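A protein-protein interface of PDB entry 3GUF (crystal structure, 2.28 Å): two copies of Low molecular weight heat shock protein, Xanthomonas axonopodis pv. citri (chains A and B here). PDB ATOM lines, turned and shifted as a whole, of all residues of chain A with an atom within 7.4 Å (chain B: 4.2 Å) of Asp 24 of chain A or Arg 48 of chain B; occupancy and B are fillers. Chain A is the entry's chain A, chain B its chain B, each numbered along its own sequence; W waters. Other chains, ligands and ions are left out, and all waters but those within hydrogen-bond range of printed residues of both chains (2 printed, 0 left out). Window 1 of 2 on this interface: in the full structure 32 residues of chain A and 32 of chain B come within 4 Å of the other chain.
Water W1 lies within hydrogen-bond range of O of Arg 64 of chain B (2.5 Å) and OD2 of Asp 11 of chain A (2.5 Å). Water W2 bridges N of Arg 65 of chain B and OD2 of Asp 24 of chain A.
Among the printed residues, merely in contact across the chains: Asn 90 of chain A with Pro 26 of chain B (3.1 Å), Val 92 of chain A with Arg 48 of chain B (3.2 Å), Arg 9 of chain A with Arg 64 of chain B (3.3 Å), Asp 24 of chain A with Pro 26 of chain B (3.5 Å), Val 92 of chain A with Arg 64 of chain B (3.6 Å), Pro 26 of chain A with Pro 26 of chain B (3.6 Å), Gly 91 of chain A with Pro 26 of chain B (3.7 Å) and Val 92 of chain A with Pro 26 of chain B (3.8 Å).
OD2 of Asp 11 of chain A is in salt-bridge range of NH2 of Arg 64 of chain B (2.8 Å). The guanidinium group (NE) of Arg 64 of chain B sits close to the backbone carbonyl oxygen (O) of Tyr 22 of chain A (3.5 Å). The side-chain carboxylate of Asp 24 of chain A lies within salt-bridge range of the guanidinium group of Arg 48 of chain B. The side-chain carboxylate of Asp 24 of chain A is in salt-bridge range of the guanidinium group of Arg 64 of chain B (3.4 Å). The side-chain amide oxygen of Asn 90 of chain A lies close to the backbone carbonyl oxygen of Ile 28 of chain B (3.1 Å).
Arg 48 of chain B touches just these residues of chain A: Asp 24 and Val 92. Printed residues of chain A within 4 Å of Ile 28 of chain B: Asn 90. Of the printed residues of chain B, Asn 90 of chain A touches Pro 26 and Ile 28. Printed residues of chain B within 4 Å of Gly 91 of chain A: Pro 26. Of the printed residues of chain A, Pro 26 of chain B touches Asp 24, Pro 26, Asn 90, Gly 91 and Val 92. Of the printed residues of chain B, Tyr 22 of chain A touches Arg 64. Leu 25 of chain A touches none of the printed residues of chain B. Arg 89 of chain A touches none of the printed residues of chain B. The nearest printed residue of chain B that does not touch Asp 24 of chain A is Arg 65 of chain B (4.8 Å). The nearest residue of chain A that does not touch Arg 48 of chain B is Arg 9 of chain A (6.1 Å).
O of Arg 9 of chain A lies within hydrogen-bond range of N of Asp 24 of chain A (2.8 Å). O of Gly 91 of chain A is in hydrogen-bond range of N of Leu 25 of chain A, at 2.6 Å. The backbone carbonyl oxygen (O) of Pro 26 of chain A sits at hydrogen-bond distance from the guanidinium group (NE) of Arg 48 of chain A (3.0 Å). The backbone carbonyl oxygen (O) of Pro 26 of chain B lies within hydrogen-bond range of the guanidinium group (NE) of Arg 48 of chain B (3.0 Å). The guanidinium group (NH1) of Arg 48 of chain B is in hydrogen-bond range of the backbone carbonyl oxygen (O) of Arg 65 of chain B (2.9 Å). The backbone carbonyl oxygen (O) of Arg 48 of chain B sits at hydrogen-bond distance from the backbone NH (N) of Gly 67 of chain B (2.5 Å).
Of the 22 printed residues of chain A, 8 touch a printed residue of chain B. Printed residues of chain A that touch a printed residue of chain B: Arg 9, Asp 11, Tyr 22, Asp 24, Pro 26, Asn 90, Gly 91 and Val 92. Hydrophobic or aromatic side chains of chain A within 4 Å of the printed part of chain B: Tyr 22, Pro 26 and Val 92. Of the 10 printed residues of chain B, 4 touch a printed residue of chain A. Among the printed residues, 13 pairs touch across the chains. Among the printed residues, Asp or Glu carboxylates within 4 Å of a Lys or Arg side-chain nitrogen of the other chain: Asp 11 of chain A with Arg 64 of chain B, Asp 24 of chain A with Arg 48 of chain B and Asp 24 of chain A with Arg 64 of chain B.
Pro 26 of chain B touches its own counterpart, Pro 26 of chain A. Positions printed for both chains: 6, 26, 28 and 48. Of the 13 pairs that touch across the chains among the printed residues, 1 has its exchanged pair printed and touching as well.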
ATOM      1  N   TRP A   6     -10.450   3.168 -33.762  1.00  0.00           N
ATOM      2  CA  TRP A   6      -9.783   3.816 -32.627  1.00  0.00           C
ATOM      3  C   TRP A   6      -8.252   3.897 -32.834  1.00  0.00           C
ATOM      4  O   TRP A   6      -7.644   3.128 -33.580  1.00  0.00           O
ATOM      5  CB  TRP A   6     -10.132   3.166 -31.265  1.00  0.00           C
ATOM      6  CG  TRP A   6      -9.550   1.863 -30.972  1.00  0.00           C
ATOM      7  CD1 TRP A   6      -9.605   0.753 -31.759  1.00  0.00           C
ATOM      8  CD2 TRP A   6      -8.901   1.454 -29.737  1.00  0.00           C
ATOM      9  NE1 TRP A   6      -8.956  -0.324 -31.130  1.00  0.00           N
ATOM     10  CE2 TRP A   6      -8.532   0.087 -29.883  1.00  0.00           C
ATOM     11  CE3 TRP A   6      -8.574   2.115 -28.548  1.00  0.00           C
ATOM     12  CZ2 TRP A   6      -7.847  -0.631 -28.883  1.00  0.00           C
ATOM     13  CZ3 TRP A   6      -7.910   1.384 -27.542  1.00  0.00           C
ATOM     14  CH2 TRP A   6      -7.526   0.044 -27.736  1.00  0.00           C
ATOM     15  N   VAL A   7      -7.646   4.844 -32.136  1.00  0.00           N
ATOM     16  CA  VAL A   7      -6.205   4.981 -32.147  1.00  0.00           C
ATOM     17  C   VAL A   7      -5.708   4.644 -30.755  1.00  0.00           C
ATOM     18  O   VAL A   7      -5.700   5.524 -29.917  1.00  0.00           O
ATOM     19  CB  VAL A   7      -5.840   6.432 -32.646  1.00  0.00           C
ATOM     20  CG1 VAL A   7      -4.449   6.502 -33.066  1.00  0.00           C
ATOM     21  CG2 VAL A   7      -6.749   6.802 -33.848  1.00  0.00           C
ATOM     22  N   PRO A   8      -5.341   3.370 -30.465  1.00  0.00           N
ATOM     23  CA  PRO A   8      -4.614   3.096 -29.218  1.00  0.00           C
ATOM     24  C   PRO A   8      -3.365   3.927 -29.117  1.00  0.00           C
ATOM     25  O   PRO A   8      -2.781   4.244 -30.151  1.00  0.00           O
ATOM     26  CB  PRO A   8      -4.167   1.652 -29.352  1.00  0.00           C
ATOM     27  CG  PRO A   8      -4.976   1.065 -30.346  1.00  0.00           C
ATOM     28  CD  PRO A   8      -5.568   2.133 -31.216  1.00  0.00           C
ATOM     29  N   ARG A   9      -2.980   4.248 -27.879  1.00  0.00           N
ATOM     30  CA  ARG A   9      -1.863   5.107 -27.561  1.00  0.00           C
ATOM     31  C   ARG A   9      -0.594   4.321 -27.703  1.00  0.00           C
ATOM     32  O   ARG A   9      -0.451   3.236 -27.081  1.00  0.00           O
ATOM     33  CB  ARG A   9      -1.881   5.434 -26.063  1.00  0.00           C
ATOM     34  CG  ARG A   9      -3.085   6.191 -25.551  1.00  0.00           C
ATOM     35  CD  ARG A   9      -3.392   7.264 -26.434  1.00  0.00           C
ATOM     36  NE  ARG A   9      -4.174   8.279 -25.728  1.00  0.00           N
ATOM     37  CZ  ARG A   9      -4.952   9.120 -26.379  1.00  0.00           C
ATOM     38  NH1 ARG A   9      -5.042   8.959 -27.711  1.00  0.00           N
ATOM     39  NH2 ARG A   9      -5.641  10.062 -25.728  1.00  0.00           N
ATOM     40  N   VAL A  10       0.374   4.913 -28.387  1.00  0.00           N
ATOM     41  CA  VAL A  10       1.629   4.278 -28.560  1.00  0.00           C
ATOM     42  C   VAL A  10       2.693   5.288 -28.153  1.00  0.00           C
ATOM     43  O   VAL A  10       2.658   6.403 -28.608  1.00  0.00           O
ATOM     44  CB  VAL A  10       1.740   3.871 -30.015  1.00  0.00           C
ATOM     45  CG1 VAL A  10       3.131   3.305 -30.313  1.00  0.00           C
ATOM     46  CG2 VAL A  10       0.669   2.786 -30.275  1.00  0.00           C
ATOM     47  N   ASP A  11       3.613   4.898 -27.294  1.00  0.00           N
ATOM     48  CA  ASP A  11       4.811   5.662 -27.085  1.00  0.00           C
ATOM     49  C   ASP A  11       5.921   5.009 -27.908  1.00  0.00           C
ATOM     50  O   ASP A  11       6.008   3.768 -28.028  1.00  0.00           O
ATOM     51  CB  ASP A  11       5.253   5.673 -25.632  1.00  0.00           C
ATOM     52  CG  ASP A  11       4.242   6.270 -24.703  1.00  0.00           C
ATOM     53  OD1 ASP A  11       3.389   7.073 -25.149  1.00  0.00           O
ATOM     54  OD2 ASP A  11       4.278   5.876 -23.513  1.00  0.00           O
ATOM     55  N   LEU A  21       8.461   0.496 -28.750  1.00  0.00           N
ATOM     56  CA  LEU A  21       7.114   1.019 -28.874  1.00  0.00           C
ATOM     57  C   LEU A  21       6.322   0.404 -27.747  1.00  0.00           C
ATOM     58  O   LEU A  21       6.447  -0.767 -27.446  1.00  0.00           O
ATOM     59  CB  LEU A  21       6.590   0.644 -30.151  1.00  0.00           C
ATOM     60  CG  LEU A  21       7.410   1.266 -31.288  1.00  0.00           C
ATOM     61  CD1 LEU A  21       8.268   0.233 -32.055  1.00  0.00           C
ATOM     62  CD2 LEU A  21       6.384   1.852 -32.234  1.00  0.00           C
ATOM     63  N   TYR A  22       5.583   1.222 -27.066  1.00  0.00           N
ATOM     64  CA  TYR A  22       4.703   0.735 -25.964  1.00  0.00           C
ATOM     65  C   TYR A  22       3.289   1.086 -26.441  1.00  0.00           C
ATOM     66  O   TYR A  22       2.980   2.263 -26.654  1.00  0.00           O
ATOM     67  CB  TYR A  22       4.994   1.536 -24.750  1.00  0.00           C
ATOM     68  CG  TYR A  22       6.466   1.473 -24.354  1.00  0.00           C
ATOM     69  CD1 TYR A  22       6.917   0.425 -23.590  1.00  0.00           C
ATOM     70  CD2 TYR A  22       7.382   2.489 -24.704  1.00  0.00           C
ATOM     71  CE1 TYR A  22       8.177   0.320 -23.226  1.00  0.00           C
ATOM     72  CE2 TYR A  22       8.715   2.404 -24.292  1.00  0.00           C
ATOM     73  CZ  TYR A  22       9.082   1.299 -23.548  1.00  0.00           C
ATOM     74  OH  TYR A  22      10.358   1.067 -23.052  1.00  0.00           O
ATOM     75  N   ALA A  23       2.471   0.081 -26.684  1.00  0.00           N
ATOM     76  CA  ALA A  23       1.182   0.344 -27.205  1.00  0.00           C
ATOM     77  C   ALA A  23       0.172  -0.093 -26.125  1.00  0.00           C
ATOM     78  O   ALA A  23       0.196  -1.225 -25.674  1.00  0.00           O
ATOM     79  CB  ALA A  23       1.014  -0.462 -28.435  1.00  0.00           C
ATOM     80  N   ASP A  24      -0.647   0.826 -25.676  1.00  0.00           N
ATOM     81  CA  ASP A  24      -1.747   0.512 -24.771  1.00  0.00           C
ATOM     82  C   ASP A  24      -2.809  -0.123 -25.551  1.00  0.00           C
ATOM     83  O   ASP A  24      -3.541   0.556 -26.280  1.00  0.00           O
ATOM     84  CB  ASP A  24      -2.274   1.829 -24.252  1.00  0.00           C
ATOM     85  CG  ASP A  24      -1.470   2.317 -23.120  1.00  0.00           C
ATOM     86  OD1 ASP A  24      -0.612   1.529 -22.684  1.00  0.00           O
ATOM     87  OD2 ASP A  24      -1.734   3.421 -22.594  1.00  0.00           O
ATOM     88  N   LEU A  25      -2.862  -1.431 -25.488  1.00  0.00           N
ATOM     89  CA  LEU A  25      -3.937  -2.133 -26.159  1.00  0.00           C
ATOM     90  C   LEU A  25      -4.866  -2.923 -25.153  1.00  0.00           C
ATOM     91  O   LEU A  25      -4.938  -4.128 -25.210  1.00  0.00           O
ATOM     92  CB  LEU A  25      -3.304  -3.066 -27.203  1.00  0.00           C
ATOM     93  CG  LEU A  25      -2.657  -2.271 -28.359  1.00  0.00           C
ATOM     94  CD1 LEU A  25      -1.562  -3.105 -29.132  1.00  0.00           C
ATOM     95  CD2 LEU A  25      -3.758  -1.840 -29.295  1.00  0.00           C
ATOM     96  N   PRO A  26      -5.569  -2.256 -24.249  1.00  0.00           N
ATOM     97  CA  PRO A  26      -6.313  -3.206 -23.360  1.00  0.00           C
ATOM     98  C   PRO A  26      -7.435  -3.994 -24.049  1.00  0.00           C
ATOM     99  O   PRO A  26      -7.932  -3.583 -25.096  1.00  0.00           O
ATOM    100  CB  PRO A  26      -6.848  -2.319 -22.197  1.00  0.00           C
ATOM    101  CG  PRO A  26      -6.672  -0.933 -22.563  1.00  0.00           C
ATOM    102  CD  PRO A  26      -5.835  -0.849 -23.921  1.00  0.00           C
ATOM    103  N   GLY A  27      -7.724  -5.194 -23.547  1.00  0.00           N
ATOM    104  CA  GLY A  27      -8.885  -5.930 -23.981  1.00  0.00           C
ATOM    105  C   GLY A  27      -8.649  -6.712 -25.218  1.00  0.00           C
ATOM    106  O   GLY A  27      -9.601  -7.243 -25.837  1.00  0.00           O
ATOM    107  N   ILE A  28      -7.385  -6.788 -25.630  1.00  0.00           N
ATOM    108  CA  ILE A  28      -7.033  -7.582 -26.795  1.00  0.00           C
ATOM    109  C   ILE A  28      -6.016  -8.606 -26.367  1.00  0.00           C
ATOM    110  O   ILE A  28      -5.139  -8.333 -25.544  1.00  0.00           O
ATOM    111  CB  ILE A  28      -6.453  -6.754 -27.945  1.00  0.00           C
ATOM    112  CG1 ILE A  28      -7.372  -5.582 -28.240  1.00  0.00           C
ATOM    113  CG2 ILE A  28      -6.372  -7.612 -29.156  1.00  0.00           C
ATOM    114  CD1 ILE A  28      -6.753  -4.408 -28.856  1.00  0.00           C
ATOM    115  N   ARG A  48     -10.153  -4.265 -31.300  1.00  0.00           N
ATOM    116  CA  ARG A  48     -10.682  -4.525 -29.979  1.00  0.00           C
ATOM    117  C   ARG A  48     -12.175  -4.664 -30.091  1.00  0.00           C
ATOM    118  O   ARG A  48     -12.878  -3.763 -30.576  1.00  0.00           O
ATOM    119  CB  ARG A  48     -10.325  -3.434 -28.963  1.00  0.00           C
ATOM    120  CG  ARG A  48     -10.771  -3.725 -27.506  1.00  0.00           C
ATOM    121  CD  ARG A  48     -10.614  -2.419 -26.771  1.00  0.00           C
ATOM    122  NE  ARG A  48     -10.636  -2.400 -25.309  1.00  0.00           N
ATOM    123  CZ  ARG A  48     -10.582  -1.228 -24.671  1.00  0.00           C
ATOM    124  NH1 ARG A  48     -10.563  -0.131 -25.391  1.00  0.00           N
ATOM    125  NH2 ARG A  48     -10.598  -1.118 -23.351  1.00  0.00           N
ATOM    126  N   PHE A  69      -7.927  -1.155 -35.319  1.00  0.00           N
ATOM    127  CA  PHE A  69      -6.941  -0.109 -35.188  1.00  0.00           C
ATOM    128  C   PHE A  69      -5.759  -0.451 -36.107  1.00  0.00           C
ATOM    129  O   PHE A  69      -5.445  -1.589 -36.415  1.00  0.00           O
ATOM    130  CB  PHE A  69      -6.509   0.000 -33.735  1.00  0.00           C
ATOM    131  CG  PHE A  69      -5.884  -1.243 -33.215  1.00  0.00           C
ATOM    132  CD1 PHE A  69      -4.519  -1.430 -33.295  1.00  0.00           C
ATOM    133  CD2 PHE A  69      -6.633  -2.198 -32.617  1.00  0.00           C
ATOM    134  CE1 PHE A  69      -3.939  -2.572 -32.795  1.00  0.00           C
ATOM    135  CE2 PHE A  69      -6.045  -3.377 -32.092  1.00  0.00           C
ATOM    136  CZ  PHE A  69      -4.737  -3.562 -32.199  1.00  0.00           C
ATOM    137  N   ARG A  89       1.960  -7.258 -21.663  1.00  0.00           N
ATOM    138  CA  ARG A  89       1.537  -7.577 -20.324  1.00  0.00           C
ATOM    139  C   ARG A  89       0.630  -6.478 -19.747  1.00  0.00           C
ATOM    140  O   ARG A  89       1.000  -5.300 -19.709  1.00  0.00           O
ATOM    141  CB  ARG A  89       2.764  -7.860 -19.418  1.00  0.00           C
ATOM    142  CG  ARG A  89       3.157  -6.734 -18.475  1.00  0.00           C
ATOM    143  CD  ARG A  89       4.315  -7.168 -17.566  1.00  0.00           C
ATOM    144  NE  ARG A  89       3.896  -7.563 -16.211  1.00  0.00           N
ATOM    145  CZ  ARG A  89       3.901  -6.742 -15.161  1.00  0.00           C
ATOM    146  NH1 ARG A  89       4.282  -5.468 -15.317  1.00  0.00           N
ATOM    147  NH2 ARG A  89       3.511  -7.189 -13.958  1.00  0.00           N
ATOM    148  N   ASN A  90      -0.546  -6.889 -19.251  1.00  0.00           N
ATOM    149  CA  ASN A  90      -1.545  -5.975 -18.702  1.00  0.00           C
ATOM    150  C   ASN A  90      -2.070  -5.005 -19.763  1.00  0.00           C
ATOM    151  O   ASN A  90      -2.289  -3.841 -19.505  1.00  0.00           O
ATOM    152  CB  ASN A  90      -1.008  -5.230 -17.484  1.00  0.00           C
ATOM    153  CG  ASN A  90      -0.747  -6.156 -16.282  1.00  0.00           C
ATOM    154  OD1 ASN A  90       0.129  -5.885 -15.404  1.00  0.00           O
ATOM    155  ND2 ASN A  90      -1.508  -7.231 -16.218  1.00  0.00           N
ATOM    156  N   GLY A  91      -2.268  -5.507 -20.966  1.00  0.00           N
ATOM    157  CA  GLY A  91      -2.711  -4.679 -22.066  1.00  0.00           C
ATOM    158  C   GLY A  91      -1.710  -3.682 -22.650  1.00  0.00           C
ATOM    159  O   GLY A  91      -2.078  -2.878 -23.444  1.00  0.00           O
ATOM    160  N   VAL A  92      -0.445  -3.726 -22.269  1.00  0.00           N
ATOM    161  CA  VAL A  92       0.542  -2.853 -22.875  1.00  0.00           C
ATOM    162  C   VAL A  92       1.301  -3.728 -23.743  1.00  0.00           C
ATOM    163  O   VAL A  92       1.803  -4.748 -23.287  1.00  0.00           O
ATOM    164  CB  VAL A  92       1.456  -2.220 -21.834  1.00  0.00           C
ATOM    165  CG1 VAL A  92       2.775  -1.615 -22.464  1.00  0.00           C
ATOM    166  CG2 VAL A  92       0.677  -1.071 -21.147  1.00  0.00           C
ATOM    167  N   LEU A  93       1.345  -3.411 -25.012  1.00  0.00           N
ATOM    168  CA  LEU A  93       2.194  -4.212 -25.917  1.00  0.00           C
ATOM    169  C   LEU A  93       3.516  -3.442 -26.091  1.00  0.00           C
ATOM    170  O   LEU A  93       3.525  -2.287 -26.493  1.00  0.00           O
ATOM    171  CB  LEU A  93       1.564  -4.470 -27.278  1.00  0.00           C
ATOM    172  CG  LEU A  93       2.353  -5.277 -28.296  1.00  0.00           C
ATOM    173  CD1 LEU A  93       2.202  -6.766 -28.089  1.00  0.00           C
ATOM    174  CD2 LEU A  93       1.962  -4.965 -29.670  1.00  0.00           C
ATOM    175  N   GLU A  94       4.617  -4.117 -25.796  1.00  0.00           N
ATOM    176  CA  GLU A  94       5.946  -3.564 -25.914  1.00  0.00           C
ATOM    177  C   GLU A  94       6.579  -4.201 -27.084  1.00  0.00           C
ATOM    178  O   GLU A  94       6.703  -5.394 -27.086  1.00  0.00           O
ATOM    179  CB  GLU A  94       6.790  -3.946 -24.720  1.00  0.00           C
ATOM    180  CG  GLU A  94       8.045  -3.111 -24.746  1.00  0.00           C
ATOM    181  CD  GLU A  94       8.889  -3.366 -23.537  1.00  0.00           C
ATOM    182  OE1 GLU A  94       8.352  -3.334 -22.404  1.00  0.00           O
ATOM    183  OE2 GLU A  94      10.084  -3.602 -23.724  1.00  0.00           O
ATOM    184  N   TRP B   6      -3.432  10.860 -14.467  1.00  0.00           N
ATOM    185  CA  TRP B   6      -3.966  10.184 -15.645  1.00  0.00           C
ATOM    186  C   TRP B   6      -5.490  10.096 -15.513  1.00  0.00           C
ATOM    187  O   TRP B   6      -6.020  10.394 -14.456  1.00  0.00           O
ATOM    188  CB  TRP B   6      -3.375   8.770 -15.653  1.00  0.00           C
ATOM    189  CG  TRP B   6      -3.928   7.797 -16.659  1.00  0.00           C
ATOM    190  CD1 TRP B   6      -4.505   8.080 -17.860  1.00  0.00           C
ATOM    191  CD2 TRP B   6      -3.905   6.373 -16.554  1.00  0.00           C
ATOM    192  NE1 TRP B   6      -4.861   6.920 -18.505  1.00  0.00           N
ATOM    193  CE2 TRP B   6      -4.495   5.857 -17.730  1.00  0.00           C
ATOM    194  CE3 TRP B   6      -3.463   5.481 -15.564  1.00  0.00           C
ATOM    195  CZ2 TRP B   6      -4.661   4.488 -17.953  1.00  0.00           C
ATOM    196  CZ3 TRP B   6      -3.609   4.122 -15.782  1.00  0.00           C
ATOM    197  CH2 TRP B   6      -4.211   3.636 -16.978  1.00  0.00           C
ATOM    198  N   PRO B  26      -4.372  -0.114 -18.841  1.00  0.00           N
ATOM    199  CA  PRO B  26      -3.241  -0.950 -19.289  1.00  0.00           C
ATOM    200  C   PRO B  26      -1.964  -0.641 -18.473  1.00  0.00           C
ATOM    201  O   PRO B  26      -1.714   0.510 -18.096  1.00  0.00           O
ATOM    202  CB  PRO B  26      -3.022  -0.480 -20.735  1.00  0.00           C
ATOM    203  CG  PRO B  26      -3.596   0.890 -20.772  1.00  0.00           C
ATOM    204  CD  PRO B  26      -4.831   0.770 -19.921  1.00  0.00           C
ATOM    205  N   ILE B  28      -0.965  -1.934 -15.588  1.00  0.00           N
ATOM    206  CA  ILE B  28      -1.105  -1.908 -14.128  1.00  0.00           C
ATOM    207  C   ILE B  28      -1.424  -3.312 -13.764  1.00  0.00           C
ATOM    208  O   ILE B  28      -2.171  -3.977 -14.495  1.00  0.00           O
ATOM    209  CB  ILE B  28      -2.204  -0.929 -13.636  1.00  0.00           C
ATOM    210  CG1 ILE B  28      -1.880   0.492 -14.085  1.00  0.00           C
ATOM    211  CG2 ILE B  28      -2.292  -0.886 -12.108  1.00  0.00           C
ATOM    212  CD1 ILE B  28      -3.111   1.385 -14.268  1.00  0.00           C
ATOM    213  N   GLU B  47      -2.020   4.075  -9.423  1.00  0.00           N
ATOM    214  CA  GLU B  47      -0.954   4.827 -10.054  1.00  0.00           C
ATOM    215  C   GLU B  47      -0.413   3.990 -11.202  1.00  0.00           C
ATOM    216  O   GLU B  47      -0.082   2.789 -11.038  1.00  0.00           O
ATOM    217  CB  GLU B  47       0.162   5.164  -9.057  1.00  0.00           C
ATOM    218  CG  GLU B  47       1.320   5.939  -9.695  1.00  0.00           C
ATOM    219  CD  GLU B  47       1.752   7.173  -8.913  1.00  0.00           C
ATOM    220  OE1 GLU B  47       1.798   8.275  -9.523  1.00  0.00           O
ATOM    221  OE2 GLU B  47       2.042   7.043  -7.697  1.00  0.00           O
ATOM    222  N   ARG B  48      -0.360   4.616 -12.373  1.00  0.00           N
ATOM    223  CA  ARG B  48       0.342   4.004 -13.492  1.00  0.00           C
ATOM    224  C   ARG B  48       1.664   4.726 -13.684  1.00  0.00           C
ATOM    225  O   ARG B  48       1.705   5.975 -13.739  1.00  0.00           O
ATOM    226  CB  ARG B  48      -0.493   4.099 -14.782  1.00  0.00           C
ATOM    227  CG  ARG B  48       0.251   3.687 -15.995  1.00  0.00           C
ATOM    228  CD  ARG B  48      -0.421   4.120 -17.283  1.00  0.00           C
ATOM    229  NE  ARG B  48      -0.106   3.059 -18.217  1.00  0.00           N
ATOM    230  CZ  ARG B  48      -0.351   3.026 -19.514  1.00  0.00           C
ATOM    231  NH1 ARG B  48      -0.954   3.993 -20.186  1.00  0.00           N
ATOM    232  NH2 ARG B  48       0.022   1.933 -20.123  1.00  0.00           N
ATOM    233  N   LYS B  49       2.724   3.938 -13.794  1.00  0.00           N
ATOM    234  CA  LYS B  49       4.038   4.439 -14.176  1.00  0.00           C
ATOM    235  C   LYS B  49       4.230   4.252 -15.686  1.00  0.00           C
ATOM    236  O   LYS B  49       3.565   3.412 -16.310  1.00  0.00           O
ATOM    237  CB  LYS B  49       5.135   3.719 -13.403  1.00  0.00           C
ATOM    238  CG  LYS B  49       4.810   3.541 -11.882  1.00  0.00           C
ATOM    239  CD  LYS B  49       5.055   4.838 -11.093  1.00  0.00           C
ATOM    240  CE  LYS B  49       5.525   4.577  -9.625  1.00  0.00           C
ATOM    241  NZ  LYS B  49       4.413   4.429  -8.615  1.00  0.00           N
ATOM    242  N   ARG B  64       0.902   7.836 -24.500  1.00  0.00           N
ATOM    243  CA  ARG B  64       0.366   7.092 -23.413  1.00  0.00           C
ATOM    244  C   ARG B  64       0.370   7.892 -22.120  1.00  0.00           C
ATOM    245  O   ARG B  64       1.376   8.450 -21.747  1.00  0.00           O
ATOM    246  CB  ARG B  64       1.094   5.763 -23.248  1.00  0.00           C
ATOM    247  CG  ARG B  64       0.943   4.743 -24.420  1.00  0.00           C
ATOM    248  CD  ARG B  64       1.230   3.342 -23.932  1.00  0.00           C
ATOM    249  NE  ARG B  64       2.506   3.509 -23.454  1.00  0.00           N
ATOM    250  CZ  ARG B  64       3.091   2.944 -22.419  1.00  0.00           C
ATOM    251  NH1 ARG B  64       2.552   2.003 -21.675  1.00  0.00           N
ATOM    252  NH2 ARG B  64       4.293   3.410 -22.150  1.00  0.00           N
ATOM    253  N   ARG B  65      -0.786   7.960 -21.454  1.00  0.00           N
ATOM    254  CA  ARG B  65      -0.952   8.731 -20.204  1.00  0.00           C
ATOM    255  C   ARG B  65      -0.751   7.878 -18.994  1.00  0.00           C
ATOM    256  O   ARG B  65      -0.941   6.663 -19.040  1.00  0.00           O
ATOM    257  CB  ARG B  65      -2.286   9.425 -20.145  1.00  0.00           C
ATOM    258  CG  ARG B  65      -2.515  10.345 -21.304  1.00  0.00           C
ATOM    259  CD  ARG B  65      -1.224  11.088 -21.698  1.00  0.00           C
ATOM    260  NE  ARG B  65      -1.426  11.911 -22.894  1.00  0.00           N
ATOM    261  CZ  ARG B  65      -0.412  12.511 -23.499  1.00  0.00           C
ATOM    262  NH1 ARG B  65      -0.623  13.222 -24.590  1.00  0.00           N
ATOM    263  NH2 ARG B  65       0.831  12.403 -22.991  1.00  0.00           N
ATOM    264  N   TYR B  66      -0.329   8.520 -17.912  1.00  0.00           N
ATOM    265  CA  TYR B  66       0.163   7.779 -16.783  1.00  0.00           C
ATOM    266  C   TYR B  66       0.136   8.657 -15.514  1.00  0.00           C
ATOM    267  O   TYR B  66      -0.117   9.884 -15.545  1.00  0.00           O
ATOM    268  CB  TYR B  66       1.568   7.202 -17.085  1.00  0.00           C
ATOM    269  CG  TYR B  66       2.634   8.272 -17.267  1.00  0.00           C
ATOM    270  CD1 TYR B  66       3.501   8.631 -16.219  1.00  0.00           C
ATOM    271  CD2 TYR B  66       2.758   8.954 -18.491  1.00  0.00           C
ATOM    272  CE1 TYR B  66       4.495   9.639 -16.418  1.00  0.00           C
ATOM    273  CE2 TYR B  66       3.712   9.947 -18.695  1.00  0.00           C
ATOM    274  CZ  TYR B  66       4.573  10.289 -17.665  1.00  0.00           C
ATOM    275  OH  TYR B  66       5.481  11.288 -17.899  1.00  0.00           O
ATOM    276  N   GLY B  67       0.367   8.006 -14.387  1.00  0.00           N
ATOM    277  CA  GLY B  67       0.298   8.722 -13.140  1.00  0.00           C
ATOM    278  C   GLY B  67      -0.776   8.246 -12.210  1.00  0.00           C
ATOM    279  O   GLY B  67      -1.085   7.079 -12.168  1.00  0.00           O
HETATM  280  O   HOH W   1       3.614   7.435 -21.639  1.00  0.00           O
HETATM  281  O   HOH W   2      -3.279   6.384 -21.724  1.00  0.00           O
